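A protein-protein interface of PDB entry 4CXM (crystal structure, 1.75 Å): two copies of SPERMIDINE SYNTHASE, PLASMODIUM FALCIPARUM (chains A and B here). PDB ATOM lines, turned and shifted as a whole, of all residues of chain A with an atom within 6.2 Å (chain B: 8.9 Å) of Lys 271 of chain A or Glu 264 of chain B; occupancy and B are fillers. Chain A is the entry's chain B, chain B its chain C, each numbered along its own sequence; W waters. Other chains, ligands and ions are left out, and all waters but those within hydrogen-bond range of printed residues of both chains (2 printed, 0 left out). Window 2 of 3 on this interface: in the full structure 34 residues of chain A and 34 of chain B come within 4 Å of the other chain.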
ATOM      1  N   TYR A 218      32.700 -38.579 -15.923  1.00  0.00           N
ATOM      2  CA  TYR A 218      32.629 -38.845 -17.355  1.00  0.00           C
ATOM      3  C   TYR A 218      32.813 -37.553 -18.050  1.00  0.00           C
ATOM      4  O   TYR A 218      32.114 -36.586 -17.708  1.00  0.00           O
ATOM      5  CB  TYR A 218      31.278 -39.564 -17.688  1.00  0.00           C
ATOM      6  CG  TYR A 218      31.065 -39.867 -19.186  1.00  0.00           C
ATOM      7  CD1 TYR A 218      30.558 -38.885 -20.021  1.00  0.00           C
ATOM      8  CD2 TYR A 218      31.376 -41.116 -19.757  1.00  0.00           C
ATOM      9  CE1 TYR A 218      30.367 -39.126 -21.350  1.00  0.00           C
ATOM     10  CE2 TYR A 218      31.243 -41.334 -21.134  1.00  0.00           C
ATOM     11  CZ  TYR A 218      30.677 -40.365 -21.889  1.00  0.00           C
ATOM     12  OH  TYR A 218      30.451 -40.522 -23.263  1.00  0.00           O
ATOM     13  N   LYS A 245      39.273 -30.835 -12.212  1.00  0.00           N
ATOM     14  CA  LYS A 245      39.967 -29.612 -12.027  1.00  0.00           C
ATOM     15  C   LYS A 245      41.453 -29.832 -12.044  1.00  0.00           C
ATOM     16  O   LYS A 245      42.012 -30.538 -11.175  1.00  0.00           O
ATOM     17  CB  LYS A 245      39.654 -29.099 -10.610  1.00  0.00           C
ATOM     18  CG  LYS A 245      38.230 -28.681 -10.443  1.00  0.00           C
ATOM     19  CD  LYS A 245      38.179 -27.435  -9.562  1.00  0.00           C
ATOM     20  CE  LYS A 245      36.856 -27.374  -8.832  1.00  0.00           C
ATOM     21  NZ  LYS A 245      35.730 -27.589  -9.785  1.00  0.00           N
ATOM     22  N   SER A 267      37.934 -28.510 -17.488  1.00  0.00           N
ATOM     23  CA  SER A 267      36.748 -28.614 -16.670  1.00  0.00           C
ATOM     24  C   SER A 267      35.484 -28.654 -17.543  1.00  0.00           C
ATOM     25  O   SER A 267      34.525 -29.292 -17.208  1.00  0.00           O
ATOM     26  CB  SER A 267      36.663 -27.438 -15.666  1.00  0.00           C
ATOM     27  OG  SER A 267      37.766 -27.683 -14.838  1.00  0.00           O
ATOM     28  N   ALA A 268      35.520 -27.958 -18.638  1.00  0.00           N
ATOM     29  CA  ALA A 268      34.326 -27.875 -19.512  1.00  0.00           C
ATOM     30  C   ALA A 268      33.962 -29.194 -20.053  1.00  0.00           C
ATOM     31  O   ALA A 268      32.749 -29.475 -20.274  1.00  0.00           O
ATOM     32  CB  ALA A 268      34.535 -26.881 -20.660  1.00  0.00           C
ATOM     33  N   ALA A 269      34.960 -30.042 -20.257  1.00  0.00           N
ATOM     34  CA  ALA A 269      34.711 -31.373 -20.798  1.00  0.00           C
ATOM     35  C   ALA A 269      33.752 -32.239 -20.000  1.00  0.00           C
ATOM     36  O   ALA A 269      33.104 -33.194 -20.521  1.00  0.00           O
ATOM     37  CB  ALA A 269      36.045 -32.076 -21.082  1.00  0.00           C
ATOM     38  N   PHE A 270      33.646 -31.981 -18.706  1.00  0.00           N
ATOM     39  CA  PHE A 270      32.774 -32.690 -17.800  1.00  0.00           C
ATOM     40  C   PHE A 270      31.406 -32.048 -17.563  1.00  0.00           C
ATOM     41  O   PHE A 270      30.617 -32.597 -16.756  1.00  0.00           O
ATOM     42  CB  PHE A 270      33.495 -32.759 -16.461  1.00  0.00           C
ATOM     43  CG  PHE A 270      34.747 -33.587 -16.493  1.00  0.00           C
ATOM     44  CD1 PHE A 270      35.987 -32.942 -16.763  1.00  0.00           C
ATOM     45  CD2 PHE A 270      34.731 -34.919 -16.033  1.00  0.00           C
ATOM     46  CE1 PHE A 270      37.152 -33.683 -16.713  1.00  0.00           C
ATOM     47  CE2 PHE A 270      35.920 -35.673 -15.954  1.00  0.00           C
ATOM     48  CZ  PHE A 270      37.126 -35.015 -16.305  1.00  0.00           C
ATOM     49  N   LYS A 271      31.096 -30.978 -18.305  1.00  0.00           N
ATOM     50  CA  LYS A 271      29.758 -30.387 -18.256  1.00  0.00           C
ATOM     51  C   LYS A 271      28.932 -30.989 -19.396  1.00  0.00           C
ATOM     52  O   LYS A 271      29.120 -30.615 -20.564  1.00  0.00           O
ATOM     53  CB  LYS A 271      29.840 -28.903 -18.398  1.00  0.00           C
ATOM     54  CG  LYS A 271      30.650 -28.153 -17.372  1.00  0.00           C
ATOM     55  CD  LYS A 271      30.452 -28.530 -15.954  1.00  0.00           C
ATOM     56  CE  LYS A 271      31.385 -27.612 -15.138  1.00  0.00           C
ATOM     57  NZ  LYS A 271      31.030 -28.118 -13.751  1.00  0.00           N
ATOM     58  N   LEU A 272      28.115 -31.954 -19.038  1.00  0.00           N
ATOM     59  CA  LEU A 272      27.523 -32.843 -20.011  1.00  0.00           C
ATOM     60  C   LEU A 272      26.065 -32.451 -20.283  1.00  0.00           C
ATOM     61  O   LEU A 272      25.409 -31.922 -19.438  1.00  0.00           O
ATOM     62  CB  LEU A 272      27.482 -34.247 -19.417  1.00  0.00           C
ATOM     63  CG  LEU A 272      28.833 -34.872 -18.968  1.00  0.00           C
ATOM     64  CD1 LEU A 272      28.598 -36.175 -18.226  1.00  0.00           C
ATOM     65  CD2 LEU A 272      29.715 -35.061 -20.182  1.00  0.00           C
ATOM     66  N   PRO A 273      25.535 -32.775 -21.473  1.00  0.00           N
ATOM     67  CA  PRO A 273      24.127 -32.489 -21.646  1.00  0.00           C
ATOM     68  C   PRO A 273      23.200 -32.977 -20.516  1.00  0.00           C
ATOM     69  O   PRO A 273      23.389 -34.082 -19.953  1.00  0.00           O
ATOM     70  CB  PRO A 273      23.794 -33.251 -22.942  1.00  0.00           C
ATOM     71  CG  PRO A 273      25.112 -33.205 -23.673  1.00  0.00           C
ATOM     72  CD  PRO A 273      26.131 -33.411 -22.636  1.00  0.00           C
ATOM     73  N   LEU A 277      23.361 -36.414 -17.710  1.00  0.00           N
ATOM     74  CA  LEU A 277      23.441 -36.165 -16.260  1.00  0.00           C
ATOM     75  C   LEU A 277      22.293 -36.869 -15.569  1.00  0.00           C
ATOM     76  O   LEU A 277      22.477 -37.554 -14.574  1.00  0.00           O
ATOM     77  CB  LEU A 277      23.316 -34.692 -15.995  1.00  0.00           C
ATOM     78  CG  LEU A 277      24.537 -33.979 -15.570  1.00  0.00           C
ATOM     79  CD1 LEU A 277      24.283 -32.493 -15.751  1.00  0.00           C
ATOM     80  CD2 LEU A 277      24.863 -34.299 -14.099  1.00  0.00           C
ATOM     81  N   MET B  67      20.238 -24.797 -27.236  1.00  0.00           N
ATOM     82  CA  MET B  67      21.420 -23.936 -27.016  1.00  0.00           C
ATOM     83  C   MET B  67      21.261 -22.571 -27.705  1.00  0.00           C
ATOM     84  O   MET B  67      21.596 -21.532 -27.123  1.00  0.00           O
ATOM     85  CB  MET B  67      22.711 -24.611 -27.418  1.00  0.00           C
ATOM     86  CG  MET B  67      23.060 -25.712 -26.503  1.00  0.00           C
ATOM     87  SD  MET B  67      23.432 -25.266 -24.765  1.00  0.00           S
ATOM     88  CE  MET B  67      24.932 -24.368 -24.960  1.00  0.00           C
ATOM     89  N   ASN B 220      30.169 -23.675 -28.959  1.00  0.00           N
ATOM     90  CA  ASN B 220      30.051 -24.966 -29.705  1.00  0.00           C
ATOM     91  C   ASN B 220      28.976 -25.828 -29.062  1.00  0.00           C
ATOM     92  O   ASN B 220      28.789 -25.900 -27.836  1.00  0.00           O
ATOM     93  CB  ASN B 220      31.325 -25.730 -29.604  1.00  0.00           C
ATOM     94  CG  ASN B 220      31.445 -26.832 -30.662  1.00  0.00           C
ATOM     95  OD1 ASN B 220      31.021 -26.681 -31.829  1.00  0.00           O
ATOM     96  ND2 ASN B 220      31.983 -27.910 -30.254  1.00  0.00           N
ATOM     97  N   SER B 222      27.366 -29.890 -29.275  1.00  0.00           N
ATOM     98  CA  SER B 222      27.504 -31.294 -29.716  1.00  0.00           C
ATOM     99  C   SER B 222      26.163 -31.769 -30.297  1.00  0.00           C
ATOM    100  O   SER B 222      25.125 -31.698 -29.620  1.00  0.00           O
ATOM    101  CB  SER B 222      27.837 -32.182 -28.558  1.00  0.00           C
ATOM    102  OG  SER B 222      27.815 -33.562 -28.929  1.00  0.00           O
ATOM    103  N   THR B 244      28.346 -15.226 -22.141  1.00  0.00           N
ATOM    104  CA  THR B 244      28.870 -16.462 -21.524  1.00  0.00           C
ATOM    105  C   THR B 244      28.347 -16.764 -20.146  1.00  0.00           C
ATOM    106  O   THR B 244      28.489 -17.899 -19.691  1.00  0.00           O
ATOM    107  CB  THR B 244      30.400 -16.498 -21.427  1.00  0.00           C
ATOM    108  OG1 THR B 244      30.806 -15.506 -20.535  1.00  0.00           O
ATOM    109  CG2 THR B 244      31.087 -16.217 -22.701  1.00  0.00           C
ATOM    110  N   LYS B 245      27.722 -15.784 -19.524  1.00  0.00           N
ATOM    111  CA  LYS B 245      27.194 -15.966 -18.163  1.00  0.00           C
ATOM    112  C   LYS B 245      25.727 -15.606 -18.078  1.00  0.00           C
ATOM    113  O   LYS B 245      25.311 -14.423 -18.161  1.00  0.00           O
ATOM    114  CB  LYS B 245      27.974 -15.083 -17.200  1.00  0.00           C
ATOM    115  CG  LYS B 245      29.468 -15.364 -17.100  1.00  0.00           C
ATOM    116  CD  LYS B 245      30.082 -14.167 -16.375  1.00  0.00           C
ATOM    117  CE  LYS B 245      31.555 -13.955 -16.673  1.00  0.00           C
ATOM    118  NZ  LYS B 245      32.342 -14.807 -15.746  1.00  0.00           N
ATOM    119  N   PRO B 246      24.896 -16.627 -17.845  1.00  0.00           N
ATOM    120  CA  PRO B 246      23.539 -16.348 -17.620  1.00  0.00           C
ATOM    121  C   PRO B 246      23.182 -15.503 -16.409  1.00  0.00           C
ATOM    122  O   PRO B 246      23.806 -15.552 -15.397  1.00  0.00           O
ATOM    123  CB  PRO B 246      22.858 -17.714 -17.578  1.00  0.00           C
ATOM    124  CG  PRO B 246      23.988 -18.721 -17.550  1.00  0.00           C
ATOM    125  CD  PRO B 246      25.267 -18.030 -17.702  1.00  0.00           C
ATOM    126  N   LYS B 248      19.971 -15.691 -15.359  1.00  0.00           N
ATOM    127  CA  LYS B 248      18.797 -16.393 -14.831  1.00  0.00           C
ATOM    128  C   LYS B 248      19.036 -17.913 -15.007  1.00  0.00           C
ATOM    129  O   LYS B 248      19.900 -18.301 -15.829  1.00  0.00           O
ATOM    130  CB  LYS B 248      17.478 -15.948 -15.471  1.00  0.00           C
ATOM    131  CG  LYS B 248      17.237 -16.397 -16.883  1.00  0.00           C
ATOM    132  CD  LYS B 248      16.159 -15.586 -17.604  1.00  0.00           C
ATOM    133  CE  LYS B 248      16.597 -14.143 -17.854  1.00  0.00           C
ATOM    134  NZ  LYS B 248      15.763 -13.549 -18.958  1.00  0.00           N
ATOM    135  N   LYS B 249      18.299 -18.727 -14.242  1.00  0.00           N
ATOM    136  CA  LYS B 249      18.301 -20.187 -14.400  1.00  0.00           C
ATOM    137  C   LYS B 249      16.952 -20.639 -14.830  1.00  0.00           C
ATOM    138  O   LYS B 249      15.913 -20.048 -14.467  1.00  0.00           O
ATOM    139  CB  LYS B 249      18.751 -20.863 -13.100  1.00  0.00           C
ATOM    140  CG  LYS B 249      20.198 -20.620 -12.853  1.00  0.00           C
ATOM    141  CD  LYS B 249      20.630 -21.298 -11.573  1.00  0.00           C
ATOM    142  CE  LYS B 249      21.987 -20.772 -11.253  1.00  0.00           C
ATOM    143  NZ  LYS B 249      22.283 -21.517 -10.012  1.00  0.00           N
ATOM    144  N   TYR B 260      19.300 -30.768 -22.989  1.00  0.00           N
ATOM    145  CA  TYR B 260      20.715 -30.396 -23.211  1.00  0.00           C
ATOM    146  C   TYR B 260      21.112 -29.264 -22.281  1.00  0.00           C
ATOM    147  O   TYR B 260      22.097 -29.349 -21.442  1.00  0.00           O
ATOM    148  CB  TYR B 260      20.950 -30.022 -24.655  1.00  0.00           C
ATOM    149  CG  TYR B 260      22.395 -29.915 -25.092  1.00  0.00           C
ATOM    150  CD1 TYR B 260      23.146 -28.786 -24.814  1.00  0.00           C
ATOM    151  CD2 TYR B 260      23.025 -30.940 -25.847  1.00  0.00           C
ATOM    152  CE1 TYR B 260      24.424 -28.666 -25.212  1.00  0.00           C
ATOM    153  CE2 TYR B 260      24.300 -30.790 -26.340  1.00  0.00           C
ATOM    154  CZ  TYR B 260      25.031 -29.643 -25.970  1.00  0.00           C
ATOM    155  OH  TYR B 260      26.365 -29.473 -26.421  1.00  0.00           O
ATOM    156  N   TYR B 261      20.451 -28.126 -22.526  1.00  0.00           N
ATOM    157  CA  TYR B 261      20.857 -26.873 -21.819  1.00  0.00           C
ATOM    158  C   TYR B 261      20.723 -26.995 -20.307  1.00  0.00           C
ATOM    159  O   TYR B 261      19.765 -27.484 -19.809  1.00  0.00           O
ATOM    160  CB  TYR B 261      20.013 -25.669 -22.386  1.00  0.00           C
ATOM    161  CG  TYR B 261      20.403 -24.372 -21.749  1.00  0.00           C
ATOM    162  CD1 TYR B 261      19.816 -24.032 -20.553  1.00  0.00           C
ATOM    163  CD2 TYR B 261      21.333 -23.542 -22.293  1.00  0.00           C
ATOM    164  CE1 TYR B 261      20.185 -22.894 -19.860  1.00  0.00           C
ATOM    165  CE2 TYR B 261      21.671 -22.337 -21.684  1.00  0.00           C
ATOM    166  CZ  TYR B 261      21.061 -22.033 -20.431  1.00  0.00           C
ATOM    167  OH  TYR B 261      21.480 -20.892 -19.762  1.00  0.00           O
ATOM    168  N   ASN B 262      21.716 -26.441 -19.608  1.00  0.00           N
ATOM    169  CA  ASN B 262      21.618 -26.053 -18.181  1.00  0.00           C
ATOM    170  C   ASN B 262      22.583 -24.926 -17.945  1.00  0.00           C
ATOM    171  O   ASN B 262      23.345 -24.507 -18.826  1.00  0.00           O
ATOM    172  CB  ASN B 262      21.815 -27.286 -17.236  1.00  0.00           C
ATOM    173  CG  ASN B 262      23.156 -27.928 -17.317  1.00  0.00           C
ATOM    174  OD1 ASN B 262      24.146 -27.307 -17.594  1.00  0.00           O
ATOM    175  ND2 ASN B 262      23.195 -29.234 -16.990  1.00  0.00           N
ATOM    176  N   TYR B 263      22.630 -24.430 -16.709  1.00  0.00           N
ATOM    177  CA  TYR B 263      23.423 -23.298 -16.352  1.00  0.00           C
ATOM    178  C   TYR B 263      24.931 -23.463 -16.521  1.00  0.00           C
ATOM    179  O   TYR B 263      25.612 -22.593 -17.049  1.00  0.00           O
ATOM    180  CB  TYR B 263      23.080 -23.009 -14.888  1.00  0.00           C
ATOM    181  CG  TYR B 263      23.889 -21.913 -14.293  1.00  0.00           C
ATOM    182  CD1 TYR B 263      23.542 -20.582 -14.546  1.00  0.00           C
ATOM    183  CD2 TYR B 263      24.901 -22.194 -13.409  1.00  0.00           C
ATOM    184  CE1 TYR B 263      24.222 -19.542 -13.949  1.00  0.00           C
ATOM    185  CE2 TYR B 263      25.617 -21.161 -12.797  1.00  0.00           C
ATOM    186  CZ  TYR B 263      25.272 -19.841 -13.078  1.00  0.00           C
ATOM    187  OH  TYR B 263      25.961 -18.826 -12.478  1.00  0.00           O
ATOM    188  N   GLU B 264      25.476 -24.627 -16.143  1.00  0.00           N
ATOM    189  CA  GLU B 264      26.907 -24.887 -16.332  1.00  0.00           C
ATOM    190  C   GLU B 264      27.218 -25.102 -17.797  1.00  0.00           C
ATOM    191  O   GLU B 264      28.241 -24.723 -18.271  1.00  0.00           O
ATOM    192  CB  GLU B 264      27.316 -26.130 -15.569  1.00  0.00           C
ATOM    193  CG  GLU B 264      27.105 -25.910 -14.085  1.00  0.00           C
ATOM    194  CD  GLU B 264      27.970 -26.798 -13.266  1.00  0.00           C
ATOM    195  OE1 GLU B 264      27.961 -28.049 -13.495  1.00  0.00           O
ATOM    196  OE2 GLU B 264      28.712 -26.221 -12.427  1.00  0.00           O
ATOM    197  N   ASN B 265      26.377 -25.830 -18.466  1.00  0.00           N
ATOM    198  CA  ASN B 265      26.624 -26.063 -19.919  1.00  0.00           C
ATOM    199  C   ASN B 265      26.632 -24.832 -20.818  1.00  0.00           C
ATOM    200  O   ASN B 265      27.292 -24.783 -21.850  1.00  0.00           O
ATOM    201  CB  ASN B 265      25.460 -26.988 -20.459  1.00  0.00           C
ATOM    202  CG  ASN B 265      25.576 -28.407 -19.914  1.00  0.00           C
ATOM    203  OD1 ASN B 265      26.541 -28.740 -19.230  1.00  0.00           O
ATOM    204  ND2 ASN B 265      24.545 -29.227 -20.135  1.00  0.00           N
ATOM    205  N   HIS B 266      25.850 -23.844 -20.427  1.00  0.00           N
ATOM    206  CA  HIS B 266      25.856 -22.537 -21.059  1.00  0.00           C
ATOM    207  C   HIS B 266      27.309 -22.015 -21.129  1.00  0.00           C
ATOM    208  O   HIS B 266      27.772 -21.681 -22.171  1.00  0.00           O
ATOM    209  CB  HIS B 266      24.930 -21.612 -20.276  1.00  0.00           C
ATOM    210  CG  HIS B 266      24.818 -20.233 -20.785  1.00  0.00           C
ATOM    211  ND1 HIS B 266      23.618 -19.582 -20.913  1.00  0.00           N
ATOM    212  CD2 HIS B 266      25.765 -19.347 -21.190  1.00  0.00           C
ATOM    213  CE1 HIS B 266      23.823 -18.360 -21.332  1.00  0.00           C
ATOM    214  NE2 HIS B 266      25.113 -18.188 -21.519  1.00  0.00           N
ATOM    215  N   SER B 267      27.943 -21.832 -19.980  1.00  0.00           N
ATOM    216  CA  SER B 267      29.292 -21.333 -19.957  1.00  0.00           C
ATOM    217  C   SER B 267      30.342 -22.277 -20.557  1.00  0.00           C
ATOM    218  O   SER B 267      31.234 -21.809 -21.224  1.00  0.00           O
ATOM    219  CB  SER B 267      29.706 -20.942 -18.518  1.00  0.00           C
ATOM    220  OG  SER B 267      28.828 -19.872 -18.185  1.00  0.00           O
ATOM    221  N   ALA B 268      30.149 -23.549 -20.465  1.00  0.00           N
ATOM    222  CA  ALA B 268      31.112 -24.533 -20.934  1.00  0.00           C
ATOM    223  C   ALA B 268      31.165 -24.532 -22.440  1.00  0.00           C
ATOM    224  O   ALA B 268      32.197 -24.721 -22.957  1.00  0.00           O
ATOM    225  CB  ALA B 268      30.757 -25.878 -20.410  1.00  0.00           C
ATOM    226  N   ALA B 269      30.030 -24.222 -23.100  1.00  0.00           N
ATOM    227  CA  ALA B 269      29.972 -24.121 -24.533  1.00  0.00           C
ATOM    228  C   ALA B 269      30.949 -23.142 -25.179  1.00  0.00           C
ATOM    229  O   ALA B 269      31.351 -23.282 -26.337  1.00  0.00           O
ATOM    230  CB  ALA B 269      28.533 -23.840 -24.971  1.00  0.00           C
ATOM    231  N   PHE B 270      31.361 -22.169 -24.393  1.00  0.00           N
ATOM    232  CA  PHE B 270      32.243 -21.149 -24.862  1.00  0.00           C
ATOM    233  C   PHE B 270      33.696 -21.428 -24.570  1.00  0.00           C
ATOM    234  O   PHE B 270      34.538 -20.611 -24.992  1.00  0.00           O
ATOM    235  CB  PHE B 270      31.892 -19.788 -24.251  1.00  0.00           C
ATOM    236  CG  PHE B 270      30.568 -19.221 -24.666  1.00  0.00           C
ATOM    237  CD1 PHE B 270      29.418 -19.546 -23.990  1.00  0.00           C
ATOM    238  CD2 PHE B 270      30.514 -18.276 -25.716  1.00  0.00           C
ATOM    239  CE1 PHE B 270      28.214 -19.004 -24.340  1.00  0.00           C
ATOM    240  CE2 PHE B 270      29.274 -17.730 -26.063  1.00  0.00           C
ATOM    241  CZ  PHE B 270      28.133 -18.094 -25.364  1.00  0.00           C
ATOM    242  N   LYS B 271      34.012 -22.573 -23.996  1.00  0.00           N
ATOM    243  CA  LYS B 271      35.404 -22.986 -23.761  1.00  0.00           C
ATOM    244  C   LYS B 271      35.903 -23.831 -24.931  1.00  0.00           C
ATOM    245  O   LYS B 271      35.513 -25.021 -25.091  1.00  0.00           O
ATOM    246  CB  LYS B 271      35.438 -23.718 -22.485  1.00  0.00           C
ATOM    247  CG  LYS B 271      34.900 -22.965 -21.260  1.00  0.00           C
ATOM    248  CD  LYS B 271      35.611 -21.610 -21.118  1.00  0.00           C
ATOM    249  CE  LYS B 271      35.157 -20.788 -19.904  1.00  0.00           C
ATOM    250  NZ  LYS B 271      34.466 -21.596 -18.893  1.00  0.00           N
HETATM  251  O   HOH W   1      27.257 -29.682 -22.497  1.00  0.00           O
HETATM  252  O   HOH W   2      26.089 -29.942 -16.903  1.00  0.00           O
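Among the printed residues, pairs that only touch across the chains: Ala 268 of chain A with Ala 268 of chain B, Ala 268 of chain A with Lys 271 of chain B, Lys 271 of chain A with Ala 268 of chain B, Pro 273 of chain A with Tyr 260 of chain B, Pro 273 of chain A with Asn 265 of chain B and Leu 277 of chain A with Asn 262 of chain B.
Ala 268 of chain B touches its own counterpart, Ala 268 of chain A. Ala 268 of chain A touches Lys 271 of chain B, and with the chains exchanged Lys 271 of chain A touches Ala 268 of chain B. 6 positions are printed for both chains. Of the 9 pairs that touch across the chains among the printed residues, 3 have their exchanged pair printed and touching as well.
The side-chain amide oxygen (OD1) of Asn 262 of chain B sits at hydrogen-bond distance from the backbone NH (N) of Asn 265 of chain B, 2.8 Å away. The backbone carbonyl oxygen of Tyr 260 of chain B is in hydrogen-bond range of the side-chain amide nitrogen of Asn 265 of chain B (2.8 Å). The backbone NH of Ser 222 of chain B sits at hydrogen-bond distance from the side-chain hydroxyl of Tyr 260 of chain B (3.1 Å). OD1 of Asn 262 of chain B lies within hydrogen-bond range of N of Glu 264 of chain B (3.3 Å).
Water W2 lies within hydrogen-bond range of OD1 of Asn 265 of chain B (2.7 Å), ND2 of Asn 262 of chain B (3.0 Å) and O of Leu 272 of chain A (3.3 Å). Water W1 bridges the backbone carbonyl oxygen (O) of Lys 271 of chain A and the side-chain amide oxygen (OD1) of Asn 265 of chain B.
Lys 245 of chain A touches none of the printed residues of chain B. Of chain B, only Glu 264, Asn 265 and Ala 268 come within 4 Å of Lys 271 of chain A. Of the printed residues of chain A, Tyr 260 of chain B touches Pro 273. Of chain A, only Lys 271 (3.1 Å) comes within 4 Å of Glu 264 of chain B. Of the printed residues of chain A, Asn 265 of chain B touches Lys 271 (3.3 Å), Leu 272 (2.9 Å) and Pro 273 (3.6 Å). The nearest residue of chain B that does not touch Lys 271 of chain A is Asn 262 of chain B (6.0 Å). The nearest printed residue of chain A that does not touch Glu 264 of chain B is Leu 277 of chain A (6.2 Å).
The backbone carbonyl oxygen (O) of Lys 271 of chain A sits close to the side-chain amide oxygen (OD1) of Asn 265 of chain B (3.5 Å). The side-chain amino group (NZ) of Lys 271 of chain A lies within salt-bridge range of the side-chain carboxylate (OE1) of Glu 264 of chain B, at 3.1 Å. O of Leu 272 of chain A sits at hydrogen-bond distance from ND2 of Asn 265 of chain B, at 2.9 Å.
Hydrophobic or aromatic side chains of chain A that line the printed part of chain B: Ala 268, Pro 273 and Leu 277. Printed residues of chain B that touch a printed residue of chain A: Tyr 260, Asn 262, Glu 264, Asn 265, Ala 268 and Lys 271. Hydrophobic or aromatic side chains of chain B that line the printed part of chain A: Tyr 260 and Ala 268. Along chain B the printed residues that touch a printed residue of chain A span positions 260 to 271. Among the printed residues, Asp or Glu carboxylates within 4 Å of a Lys or Arg side-chain nitrogen of the other chain: Lys 271 of chain A with Glu 264 of chain B (3.1 Å).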
